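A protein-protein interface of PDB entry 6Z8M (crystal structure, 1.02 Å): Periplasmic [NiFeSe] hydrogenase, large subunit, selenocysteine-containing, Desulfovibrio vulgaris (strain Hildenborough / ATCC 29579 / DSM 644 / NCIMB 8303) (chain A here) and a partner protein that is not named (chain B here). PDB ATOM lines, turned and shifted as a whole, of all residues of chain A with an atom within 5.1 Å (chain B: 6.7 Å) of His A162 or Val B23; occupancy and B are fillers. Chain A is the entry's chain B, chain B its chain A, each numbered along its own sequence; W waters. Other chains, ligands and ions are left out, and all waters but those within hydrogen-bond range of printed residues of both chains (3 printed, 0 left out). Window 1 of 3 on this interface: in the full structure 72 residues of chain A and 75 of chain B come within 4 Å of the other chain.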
ATOM      1  N   GLY A  65     -20.291  17.099   4.259  1.00  0.00           N
ATOM      2  CA  GLY A  65     -21.139  16.390   3.324  1.00  0.00           C
ATOM      3  C   GLY A  65     -22.110  17.243   2.550  1.00  0.00           C
ATOM      4  O   GLY A  65     -22.860  16.710   1.726  1.00  0.00           O
ATOM      5  N   VAL A  66     -22.112  18.546   2.810  1.00  0.00           N
ATOM      6  CA  VAL A  66     -22.830  19.512   1.989  1.00  0.00           C
ATOM      7  C   VAL A  66     -21.987  19.954   0.800  1.00  0.00           C
ATOM      8  O   VAL A  66     -22.500  20.053  -0.318  1.00  0.00           O
ATOM      9  CB  VAL A  66     -23.305  20.721   2.829  1.00  0.00           C
ATOM     10  CG1 VAL A  66     -24.035  21.726   1.938  1.00  0.00           C
ATOM     11  CG2 VAL A  66     -24.175  20.272   3.996  1.00  0.00           C
ATOM     12  N   ASN A 102     -23.121  20.375  -8.035  1.00  0.00           N
ATOM     13  CA  ASN A 102     -23.305  20.602  -6.611  1.00  0.00           C
ATOM     14  C   ASN A 102     -23.423  22.074  -6.259  1.00  0.00           C
ATOM     15  O   ASN A 102     -23.994  22.383  -5.215  1.00  0.00           O
ATOM     16  CB  ASN A 102     -22.260  19.947  -5.704  1.00  0.00           C
ATOM     17  CG  ASN A 102     -22.808  19.751  -4.313  1.00  0.00           C
ATOM     18  OD1 ASN A 102     -23.904  19.201  -4.150  1.00  0.00           O
ATOM     19  ND2 ASN A 102     -22.091  20.213  -3.310  1.00  0.00           N
ATOM     20  N   GLN A 105     -27.076  22.306  -6.387  1.00  0.00           N
ATOM     21  CA  GLN A 105     -27.658  21.672  -5.208  1.00  0.00           C
ATOM     22  C   GLN A 105     -27.519  22.553  -3.986  1.00  0.00           C
ATOM     23  O   GLN A 105     -28.463  22.709  -3.208  1.00  0.00           O
ATOM     24  CB  GLN A 105     -26.963  20.338  -4.914  1.00  0.00           C
ATOM     25  CG  GLN A 105     -27.614  19.583  -3.740  1.00  0.00           C
ATOM     26  CD  GLN A 105     -27.075  19.867  -2.331  1.00  0.00           C
ATOM     27  OE1 GLN A 105     -27.799  19.678  -1.361  1.00  0.00           O
ATOM     28  NE2 GLN A 105     -25.799  20.223  -2.197  1.00  0.00           N
ATOM     29  N   ARG A 158     -33.197  19.713  -5.508  1.00  0.00           N
ATOM     30  CA  ARG A 158     -31.840  19.505  -4.996  1.00  0.00           C
ATOM     31  C   ARG A 158     -31.438  18.041  -5.059  1.00  0.00           C
ATOM     32  O   ARG A 158     -30.257  17.740  -5.263  1.00  0.00           O
ATOM     33  CB  ARG A 158     -31.654  20.082  -3.581  1.00  0.00           C
ATOM     34  CG  ARG A 158     -32.501  19.447  -2.480  1.00  0.00           C
ATOM     35  CD  ARG A 158     -31.788  19.421  -1.124  1.00  0.00           C
ATOM     36  NE  ARG A 158     -30.502  18.739  -1.205  1.00  0.00           N
ATOM     37  CZ  ARG A 158     -30.354  17.434  -1.416  1.00  0.00           C
ATOM     38  NH1 ARG A 158     -31.400  16.627  -1.488  1.00  0.00           N
ATOM     39  NH2 ARG A 158     -29.133  16.935  -1.537  1.00  0.00           N
ATOM     40  N   ARG A 159     -32.400  17.127  -4.897  1.00  0.00           N
ATOM     41  CA  ARG A 159     -32.107  15.704  -5.027  1.00  0.00           C
ATOM     42  C   ARG A 159     -31.695  15.377  -6.456  1.00  0.00           C
ATOM     43  O   ARG A 159     -30.737  14.626  -6.682  1.00  0.00           O
ATOM     44  CB  ARG A 159     -33.331  14.897  -4.583  1.00  0.00           C
ATOM     45  CG  ARG A 159     -33.127  13.405  -4.707  1.00  0.00           C
ATOM     46  CD  ARG A 159     -34.372  12.607  -4.368  1.00  0.00           C
ATOM     47  NE  ARG A 159     -35.475  12.855  -5.290  1.00  0.00           N
ATOM     48  CZ  ARG A 159     -35.520  12.452  -6.556  1.00  0.00           C
ATOM     49  NH1 ARG A 159     -34.526  11.772  -7.090  1.00  0.00           N
ATOM     50  NH2 ARG A 159     -36.592  12.728  -7.300  1.00  0.00           N
ATOM     51  N   ILE A 160     -32.394  15.951  -7.431  1.00  0.00           N
ATOM     52  CA  ILE A 160     -32.046  15.765  -8.834  1.00  0.00           C
ATOM     53  C   ILE A 160     -30.646  16.300  -9.110  1.00  0.00           C
ATOM     54  O   ILE A 160     -29.884  15.714  -9.887  1.00  0.00           O
ATOM     55  CB  ILE A 160     -33.115  16.420  -9.735  1.00  0.00           C
ATOM     56  CG1 ILE A 160     -34.430  15.647  -9.633  1.00  0.00           C
ATOM     57  CG2 ILE A 160     -32.622  16.524 -11.181  1.00  0.00           C
ATOM     58  CD1 ILE A 160     -35.622  16.403 -10.222  1.00  0.00           C
ATOM     59  N   CYS A 161     -30.280  17.417  -8.476  1.00  0.00           N
ATOM     60  CA  CYS A 161     -28.916  17.921  -8.634  1.00  0.00           C
ATOM     61  C   CYS A 161     -27.889  16.894  -8.181  1.00  0.00           C
ATOM     62  O   CYS A 161     -26.838  16.749  -8.806  1.00  0.00           O
ATOM     63  CB  CYS A 161     -28.723  19.208  -7.831  1.00  0.00           C
ATOM     64  SG  CYS A 161     -29.614  20.656  -8.479  1.00  0.00           S
ATOM     65  N   HIS A 162     -28.162  16.183  -7.086  1.00  0.00           N
ATOM     66  CA  HIS A 162     -27.255  15.126  -6.652  1.00  0.00           C
ATOM     67  C   HIS A 162     -27.246  13.930  -7.597  1.00  0.00           C
ATOM     68  O   HIS A 162     -26.200  13.290  -7.743  1.00  0.00           O
ATOM     69  CB  HIS A 162     -27.529  14.724  -5.209  1.00  0.00           C
ATOM     70  CG  HIS A 162     -26.750  15.532  -4.230  1.00  0.00           C
ATOM     71  ND1 HIS A 162     -26.736  15.245  -2.883  1.00  0.00           N
ATOM     72  CD2 HIS A 162     -25.971  16.627  -4.405  1.00  0.00           C
ATOM     73  CE1 HIS A 162     -25.943  16.113  -2.280  1.00  0.00           C
ATOM     74  NE2 HIS A 162     -25.477  16.963  -3.177  1.00  0.00           N
ATOM     75  N   GLU A 163     -28.362  13.626  -8.270  1.00  0.00           N
ATOM     76  CA  GLU A 163     -28.301  12.642  -9.347  1.00  0.00           C
ATOM     77  C   GLU A 163     -27.354  13.113 -10.442  1.00  0.00           C
ATOM     78  O   GLU A 163     -26.574  12.325 -10.980  1.00  0.00           O
ATOM     79  CB  GLU A 163     -29.689  12.392  -9.929  1.00  0.00           C
ATOM     80  CG  GLU A 163     -30.634  11.773  -8.925  1.00  0.00           C
ATOM     81  CD  GLU A 163     -31.928  11.267  -9.529  1.00  0.00           C
ATOM     82  OE1 GLU A 163     -32.232  11.632 -10.680  1.00  0.00           O
ATOM     83  OE2 GLU A 163     -32.649  10.515  -8.836  1.00  0.00           O
ATOM     84  N   MET A 164     -27.396  14.398 -10.782  1.00  0.00           N
ATOM     85  CA  MET A 164     -26.452  14.930 -11.757  1.00  0.00           C
ATOM     86  C   MET A 164     -25.014  14.735 -11.305  1.00  0.00           C
ATOM     87  O   MET A 164     -24.159  14.344 -12.104  1.00  0.00           O
ATOM     88  CB  MET A 164     -26.739  16.406 -12.035  1.00  0.00           C
ATOM     89  CG  MET A 164     -28.049  16.632 -12.772  1.00  0.00           C
ATOM     90  SD  MET A 164     -28.604  18.338 -12.701  1.00  0.00           S
ATOM     91  CE  MET A 164     -27.215  19.187 -13.459  1.00  0.00           C
ATOM     92  N   VAL A 165     -24.726  15.035 -10.035  1.00  0.00           N
ATOM     93  CA  VAL A 165     -23.375  14.837  -9.502  1.00  0.00           C
ATOM     94  C   VAL A 165     -22.969  13.376  -9.636  1.00  0.00           C
ATOM     95  O   VAL A 165     -21.842  13.055 -10.041  1.00  0.00           O
ATOM     96  CB  VAL A 165     -23.280  15.281  -8.029  1.00  0.00           C
ATOM     97  CG1 VAL A 165     -21.895  14.944  -7.446  1.00  0.00           C
ATOM     98  CG2 VAL A 165     -23.548  16.767  -7.879  1.00  0.00           C
ATOM     99  N   ALA A 166     -23.873  12.469  -9.269  1.00  0.00           N
ATOM    100  CA  ALA A 166     -23.533  11.057  -9.219  1.00  0.00           C
ATOM    101  C   ALA A 166     -23.374  10.430 -10.600  1.00  0.00           C
ATOM    102  O   ALA A 166     -22.699   9.400 -10.712  1.00  0.00           O
ATOM    103  CB  ALA A 166     -24.613  10.309  -8.443  1.00  0.00           C
ATOM    104  N   LEU A 167     -23.959  11.010 -11.651  1.00  0.00           N
ATOM    105  CA  LEU A 167     -23.853  10.400 -12.971  1.00  0.00           C
ATOM    106  C   LEU A 167     -22.402  10.134 -13.343  1.00  0.00           C
ATOM    107  O   LEU A 167     -22.072   9.048 -13.823  1.00  0.00           O
ATOM    108  CB  LEU A 167     -24.571  11.250 -14.019  1.00  0.00           C
ATOM    109  CG  LEU A 167     -26.079  10.984 -14.114  1.00  0.00           C
ATOM    110  CD1 LEU A 167     -26.779  12.089 -14.865  1.00  0.00           C
ATOM    111  CD2 LEU A 167     -26.349   9.637 -14.805  1.00  0.00           C
ATOM    112  N   MET A 172     -23.304  10.657  -4.188  1.00  0.00           N
ATOM    113  CA  MET A 172     -23.220  11.930  -3.488  1.00  0.00           C
ATOM    114  C   MET A 172     -24.160  11.868  -2.296  1.00  0.00           C
ATOM    115  O   MET A 172     -25.284  11.372  -2.451  1.00  0.00           O
ATOM    116  CB  MET A 172     -23.652  13.038  -4.446  1.00  0.00           C
ATOM    117  CG  MET A 172     -23.380  14.431  -3.961  1.00  0.00           C
ATOM    118  SD  MET A 172     -21.638  14.846  -3.726  1.00  0.00           S
ATOM    119  CE  MET A 172     -21.858  16.628  -3.573  1.00  0.00           C
ATOM    120  N   PRO A 173     -23.770  12.364  -1.112  1.00  0.00           N
ATOM    121  CA  PRO A 173     -22.459  12.894  -0.730  1.00  0.00           C
ATOM    122  C   PRO A 173     -21.309  11.913  -0.945  1.00  0.00           C
ATOM    123  O   PRO A 173     -21.475  10.690  -0.932  1.00  0.00           O
ATOM    124  CB  PRO A 173     -22.609  13.173   0.769  1.00  0.00           C
ATOM    125  CG  PRO A 173     -24.071  13.391   0.962  1.00  0.00           C
ATOM    126  CD  PRO A 173     -24.742  12.457  -0.010  1.00  0.00           C
ATOM    127  N   TRP B  12     -32.448  14.720  16.443  1.00  0.00           N
ATOM    128  CA  TRP B  12     -31.269  14.431  15.640  1.00  0.00           C
ATOM    129  C   TRP B  12     -30.135  15.288  16.177  1.00  0.00           C
ATOM    130  O   TRP B  12     -30.159  16.517  16.036  1.00  0.00           O
ATOM    131  CB  TRP B  12     -31.575  14.749  14.184  1.00  0.00           C
ATOM    132  CG  TRP B  12     -30.532  14.308  13.200  1.00  0.00           C
ATOM    133  CD1 TRP B  12     -29.239  14.734  13.128  1.00  0.00           C
ATOM    134  CD2 TRP B  12     -30.718  13.412  12.109  1.00  0.00           C
ATOM    135  NE1 TRP B  12     -28.597  14.134  12.080  1.00  0.00           N
ATOM    136  CE2 TRP B  12     -29.488  13.320  11.431  1.00  0.00           C
ATOM    137  CE3 TRP B  12     -31.802  12.669  11.645  1.00  0.00           C
ATOM    138  CZ2 TRP B  12     -29.314  12.514  10.312  1.00  0.00           C
ATOM    139  CZ3 TRP B  12     -31.627  11.867  10.537  1.00  0.00           C
ATOM    140  CH2 TRP B  12     -30.396  11.791   9.887  1.00  0.00           C
ATOM    141  N   CYS B  18     -20.284  15.364   9.580  1.00  0.00           N
ATOM    142  CA  CYS B  18     -20.030  16.276   8.476  1.00  0.00           C
ATOM    143  C   CYS B  18     -21.317  16.754   7.826  1.00  0.00           C
ATOM    144  O   CYS B  18     -21.265  17.466   6.812  1.00  0.00           O
ATOM    145  CB  CYS B  18     -19.140  15.618   7.416  1.00  0.00           C
ATOM    146  SG  CYS B  18     -19.987  14.451   6.333  1.00  0.00           S
ATOM    147  N   THR B  19     -22.467  16.373   8.380  1.00  0.00           N
ATOM    148  CA  THR B  19     -23.795  16.673   7.875  1.00  0.00           C
ATOM    149  C   THR B  19     -24.122  15.841   6.639  1.00  0.00           C
ATOM    150  O   THR B  19     -25.247  15.916   6.109  1.00  0.00           O
ATOM    151  CB  THR B  19     -24.019  18.187   7.732  1.00  0.00           C
ATOM    152  OG1 THR B  19     -23.724  18.767   9.007  1.00  0.00           O
ATOM    153  CG2 THR B  19     -25.439  18.539   7.347  1.00  0.00           C
ATOM    154  N   GLY B  20     -23.204  14.979   6.205  1.00  0.00           N
ATOM    155  CA  GLY B  20     -23.488  14.144   5.055  1.00  0.00           C
ATOM    156  C   GLY B  20     -24.519  13.069   5.311  1.00  0.00           C
ATOM    157  O   GLY B  20     -25.177  12.608   4.374  1.00  0.00           O
ATOM    158  N   CYS B  21     -24.677  12.656   6.556  1.00  0.00           N
ATOM    159  CA  CYS B  21     -25.715  11.695   6.866  1.00  0.00           C
ATOM    160  C   CYS B  21     -27.097  12.355   6.842  1.00  0.00           C
ATOM    161  O   CYS B  21     -28.079  11.717   6.450  1.00  0.00           O
ATOM    162  CB  CYS B  21     -25.400  11.004   8.191  1.00  0.00           C
ATOM    163  SG  CYS B  21     -24.010   9.812   8.180  1.00  0.00           S
ATOM    164  N   SER B  22     -27.199  13.636   7.225  1.00  0.00           N
ATOM    165  CA  SER B  22     -28.434  14.372   6.998  1.00  0.00           C
ATOM    166  C   SER B  22     -28.686  14.569   5.507  1.00  0.00           C
ATOM    167  O   SER B  22     -29.809  14.380   5.022  1.00  0.00           O
ATOM    168  CB  SER B  22     -28.339  15.735   7.676  1.00  0.00           C
ATOM    169  OG  SER B  22     -28.426  15.636   9.079  1.00  0.00           O
ATOM    170  N   VAL B  23     -27.653  14.955   4.756  1.00  0.00           N
ATOM    171  CA  VAL B  23     -27.838  15.218   3.329  1.00  0.00           C
ATOM    172  C   VAL B  23     -28.251  13.952   2.589  1.00  0.00           C
ATOM    173  O   VAL B  23     -29.113  13.991   1.711  1.00  0.00           O
ATOM    174  CB  VAL B  23     -26.585  15.856   2.706  1.00  0.00           C
ATOM    175  CG1 VAL B  23     -26.735  15.979   1.197  1.00  0.00           C
ATOM    176  CG2 VAL B  23     -26.327  17.232   3.297  1.00  0.00           C
ATOM    177  N   THR B  24     -27.622  12.822   2.901  1.00  0.00           N
ATOM    178  CA  THR B  24     -28.005  11.598   2.207  1.00  0.00           C
ATOM    179  C   THR B  24     -29.485  11.295   2.423  1.00  0.00           C
ATOM    180  O   THR B  24     -30.183  10.859   1.500  1.00  0.00           O
ATOM    181  CB  THR B  24     -27.084  10.446   2.603  1.00  0.00           C
ATOM    182  OG1 THR B  24     -27.090   9.500   1.544  1.00  0.00           O
ATOM    183  CG2 THR B  24     -27.504   9.751   3.882  1.00  0.00           C
ATOM    184  N   LEU B  25     -29.986  11.551   3.631  1.00  0.00           N
ATOM    185  CA  LEU B  25     -31.398  11.326   3.922  1.00  0.00           C
ATOM    186  C   LEU B  25     -32.287  12.232   3.078  1.00  0.00           C
ATOM    187  O   LEU B  25     -33.342  11.804   2.593  1.00  0.00           O
ATOM    188  CB  LEU B  25     -31.645  11.537   5.415  1.00  0.00           C
ATOM    189  CG  LEU B  25     -33.112  11.457   5.845  1.00  0.00           C
ATOM    190  CD1 LEU B  25     -33.761  10.124   5.513  1.00  0.00           C
ATOM    191  CD2 LEU B  25     -33.201  11.720   7.335  1.00  0.00           C
ATOM    192  N   LEU B  26     -31.856  13.479   2.856  1.00  0.00           N
ATOM    193  CA  LEU B  26     -32.604  14.384   1.983  1.00  0.00           C
ATOM    194  C   LEU B  26     -32.749  13.832   0.572  1.00  0.00           C
ATOM    195  O   LEU B  26     -33.648  14.265  -0.163  1.00  0.00           O
ATOM    196  CB  LEU B  26     -31.918  15.742   1.898  1.00  0.00           C
ATOM    197  CG  LEU B  26     -31.726  16.530   3.192  1.00  0.00           C
ATOM    198  CD1 LEU B  26     -31.092  17.869   2.855  1.00  0.00           C
ATOM    199  CD2 LEU B  26     -33.028  16.725   3.926  1.00  0.00           C
ATOM    200  N   ASN B  27     -31.895  12.890   0.176  1.00  0.00           N
ATOM    201  CA  ASN B  27     -31.953  12.309  -1.157  1.00  0.00           C
ATOM    202  C   ASN B  27     -32.877  11.098  -1.268  1.00  0.00           C
ATOM    203  O   ASN B  27     -32.923  10.477  -2.328  1.00  0.00           O
ATOM    204  CB  ASN B  27     -30.560  11.913  -1.630  1.00  0.00           C
ATOM    205  CG  ASN B  27     -29.684  13.112  -1.938  1.00  0.00           C
ATOM    206  OD1 ASN B  27     -30.166  14.201  -2.245  1.00  0.00           O
ATOM    207  ND2 ASN B  27     -28.379  12.894  -1.893  1.00  0.00           N
ATOM    208  N   SER B  28     -33.634  10.757  -0.228  1.00  0.00           N
ATOM    209  CA  SER B  28     -34.535   9.616  -0.310  1.00  0.00           C
ATOM    210  C   SER B  28     -35.536   9.796  -1.449  1.00  0.00           C
ATOM    211  O   SER B  28     -36.152  10.852  -1.598  1.00  0.00           O
ATOM    212  CB  SER B  28     -35.273   9.480   1.016  1.00  0.00           C
ATOM    213  OG  SER B  28     -36.063   8.303   1.034  1.00  0.00           O
ATOM    214  N   THR B  48     -29.777  21.508  11.554  1.00  0.00           N
ATOM    215  CA  THR B  48     -29.595  21.968  10.186  1.00  0.00           C
ATOM    216  C   THR B  48     -30.879  22.524   9.585  1.00  0.00           C
ATOM    217  O   THR B  48     -30.809  23.383   8.707  1.00  0.00           O
ATOM    218  CB  THR B  48     -29.063  20.828   9.306  1.00  0.00           C
ATOM    219  OG1 THR B  48     -28.007  20.137   9.981  1.00  0.00           O
ATOM    220  CG2 THR B  48     -28.545  21.368   7.988  1.00  0.00           C
ATOM    221  N   GLU B  77     -25.606  11.569  14.563  1.00  0.00           N
ATOM    222  CA  GLU B  77     -24.769  11.710  13.378  1.00  0.00           C
ATOM    223  C   GLU B  77     -23.414  12.220  13.866  1.00  0.00           C
ATOM    224  O   GLU B  77     -23.350  13.266  14.511  1.00  0.00           O
ATOM    225  CB  GLU B  77     -25.410  12.723  12.415  1.00  0.00           C
ATOM    226  CG  GLU B  77     -24.521  13.211  11.258  1.00  0.00           C
ATOM    227  CD  GLU B  77     -25.260  14.067  10.242  1.00  0.00           C
ATOM    228  OE1 GLU B  77     -26.277  14.707  10.592  1.00  0.00           O
ATOM    229  OE2 GLU B  77     -24.796  14.135   9.072  1.00  0.00           O
ATOM    230  N   PRO B 160     -21.477   8.386   3.252  1.00  0.00           N
ATOM    231  CA  PRO B 160     -22.655   8.256   4.104  1.00  0.00           C
ATOM    232  C   PRO B 160     -23.405   6.944   3.847  1.00  0.00           C
ATOM    233  O   PRO B 160     -23.158   6.263   2.848  1.00  0.00           O
ATOM    234  CB  PRO B 160     -23.544   9.408   3.622  1.00  0.00           C
ATOM    235  CG  PRO B 160     -23.260   9.447   2.147  1.00  0.00           C
ATOM    236  CD  PRO B 160     -21.786   9.104   2.006  1.00  0.00           C
ATOM    237  N   PRO B 163     -29.768   6.617   1.616  1.00  0.00           N
ATOM    238  CA  PRO B 163     -31.016   7.006   2.299  1.00  0.00           C
ATOM    239  C   PRO B 163     -31.922   5.825   2.583  1.00  0.00           C
ATOM    240  O   PRO B 163     -32.616   5.800   3.610  1.00  0.00           O
ATOM    241  CB  PRO B 163     -31.672   8.006   1.332  1.00  0.00           C
ATOM    242  CG  PRO B 163     -30.994   7.784   0.017  1.00  0.00           C
ATOM    243  CD  PRO B 163     -29.584   7.387   0.380  1.00  0.00           C
ATOM    244  N   ASN B 253     -28.209   7.405  -5.600  1.00  0.00           N
ATOM    245  CA  ASN B 253     -28.741   8.633  -6.177  1.00  0.00           C
ATOM    246  C   ASN B 253     -29.711   8.327  -7.312  1.00  0.00           C
ATOM    247  O   ASN B 253     -29.526   8.737  -8.449  1.00  0.00           O
ATOM    248  CB  ASN B 253     -27.617   9.577  -6.615  1.00  0.00           C
ATOM    249  CG  ASN B 253     -26.741   9.965  -5.466  1.00  0.00           C
ATOM    250  OD1 ASN B 253     -25.691   9.362  -5.221  1.00  0.00           O
ATOM    251  ND2 ASN B 253     -27.192  10.956  -4.704  1.00  0.00           N
ATOM    252  N   VAL B 256     -28.472   5.943 -10.475  1.00  0.00           N
ATOM    253  CA  VAL B 256     -27.718   6.417 -11.637  1.00  0.00           C
ATOM    254  C   VAL B 256     -26.275   5.920 -11.671  1.00  0.00           C
ATOM    255  O   VAL B 256     -25.627   5.998 -12.720  1.00  0.00           O
ATOM    256  CB  VAL B 256     -27.739   7.949 -11.774  1.00  0.00           C
ATOM    257  CG1 VAL B 256     -29.161   8.457 -11.877  1.00  0.00           C
ATOM    258  CG2 VAL B 256     -26.976   8.628 -10.616  1.00  0.00           C
HETATM  259  O   HOH W   1     -34.077  16.966  -0.743  1.00  0.00           O
HETATM  260  O   HOH W   2     -27.422  10.102  -1.188  1.00  0.00           O
HETATM  261  O   HOH W   3     -29.809  12.121  -5.354  1.00  0.00           O
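The backbone carbonyl oxygen of Cys B18 lies within hydrogen-bond range of the backbone NH of Gly A65 (2.8 Å). NH1 of Arg A158 lies within hydrogen-bond range of OD1 of Asn B27. The side-chain amide nitrogen (ND2) of Asn B27 is in hydrogen-bond range of a ring nitrogen (ND1) of His A162. ND2 of Asn B27 lies within hydrogen-bond range of O of Met A172 (3.5 Å). N of Met A172 lies within hydrogen-bond range of OD1 of Asn B253 (2.9 Å).
The side-chain carboxylate (OE2) of Glu B77 lies close to the backbone NH (N) of Thr B19, 3.3 Å away. The backbone carbonyl oxygen (O) of Val A66 sits at hydrogen-bond distance from the side-chain amide nitrogen (ND2) of Asn A102 (3.0 Å). NE2 of His A162 is in hydrogen-bond range of OD1 of Asn A102 (2.9 Å). NE of Arg A158 is in hydrogen-bond range of OE1 of Gln A105 (2.9 Å). NE2 of His A162 sits at hydrogen-bond distance from NE2 of Gln A105, at 3.4 Å. The guanidinium group (NH2) of Arg A158 sits at hydrogen-bond distance from a ring nitrogen (ND1) of His A162, 3.2 Å away.
Val B23 touches Gly A65 (CG2 to O, 3.8 Å). Val A66 touches Thr B19 (CG2 to CG2, 3.98 Å). Val B23 touches Val A66. CG1 of Val B23 touches NH2 of Arg A158, 3.8 Å away. Arg A158 touches Leu B26 (NH1 to O, 3.5 Å). Ser B28 touches Arg A159. Val B256 touches Ala A166. CD2 of Leu A167 touches CB of Val B256 (3.7 Å). Pro A173 touches Val B23. Pro A173 touches Pro B160.
His A162 touches three residues of chain B. Printed residues of chain B within 4 Å of Ala A166: Asn B253 and Val B256. Of the printed residues of chain A, Gly B20 touches Gly A65 (3.7 Å) and Pro A173 (3.7 Å). Cys B21 touches none of the printed residues of chain A. Val B23 touches just these residues of chain A: Gly A65 (3.8 Å), Val A66 (3.8 Å), Arg A158 (3.8 Å), His A162 (3.6 Å) and Pro A173 (3.7 Å). Of the printed residues of chain A, Ser B28 touches Arg A159. The nearest residue of chain B that does not touch His A162 is Val B256 (5.5 Å). The nearest residue of chain A that does not touch Val B23 is Gln A105 (4.6 Å).
Printed residues of chain B that touch a printed residue of chain A: Cys B18, Thr B19, Gly B20, Val B23, Leu B26, Asn B27, Ser B28, Pro B160, Asn B253 and Val B256. Hydrophobic or aromatic side chains of chain B within 4 Å of the printed part of chain A: Val B23, Leu B26, Pro B160 and Val B256. Printed residues of chain A that touch a printed residue of chain B: Gly A65, Val A66, Arg A158, Arg A159, His A162, Glu A163, Ala A166, Leu A167, Met A172 and Pro A173.
Water W2 lies within hydrogen-bond range of O of Met A172 (2.8 Å), OG1 of Thr B24 (2.8 Å) and ND2 of Asn B27 (3.0 Å). Water W1 bridges O of Leu B26 (2.8 Å) and NH1 of Arg A158 (2.8 Å). Water W3 bridges the side-chain amide nitrogen of Asn B253 and the backbone carbonyl oxygen of Arg A159.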
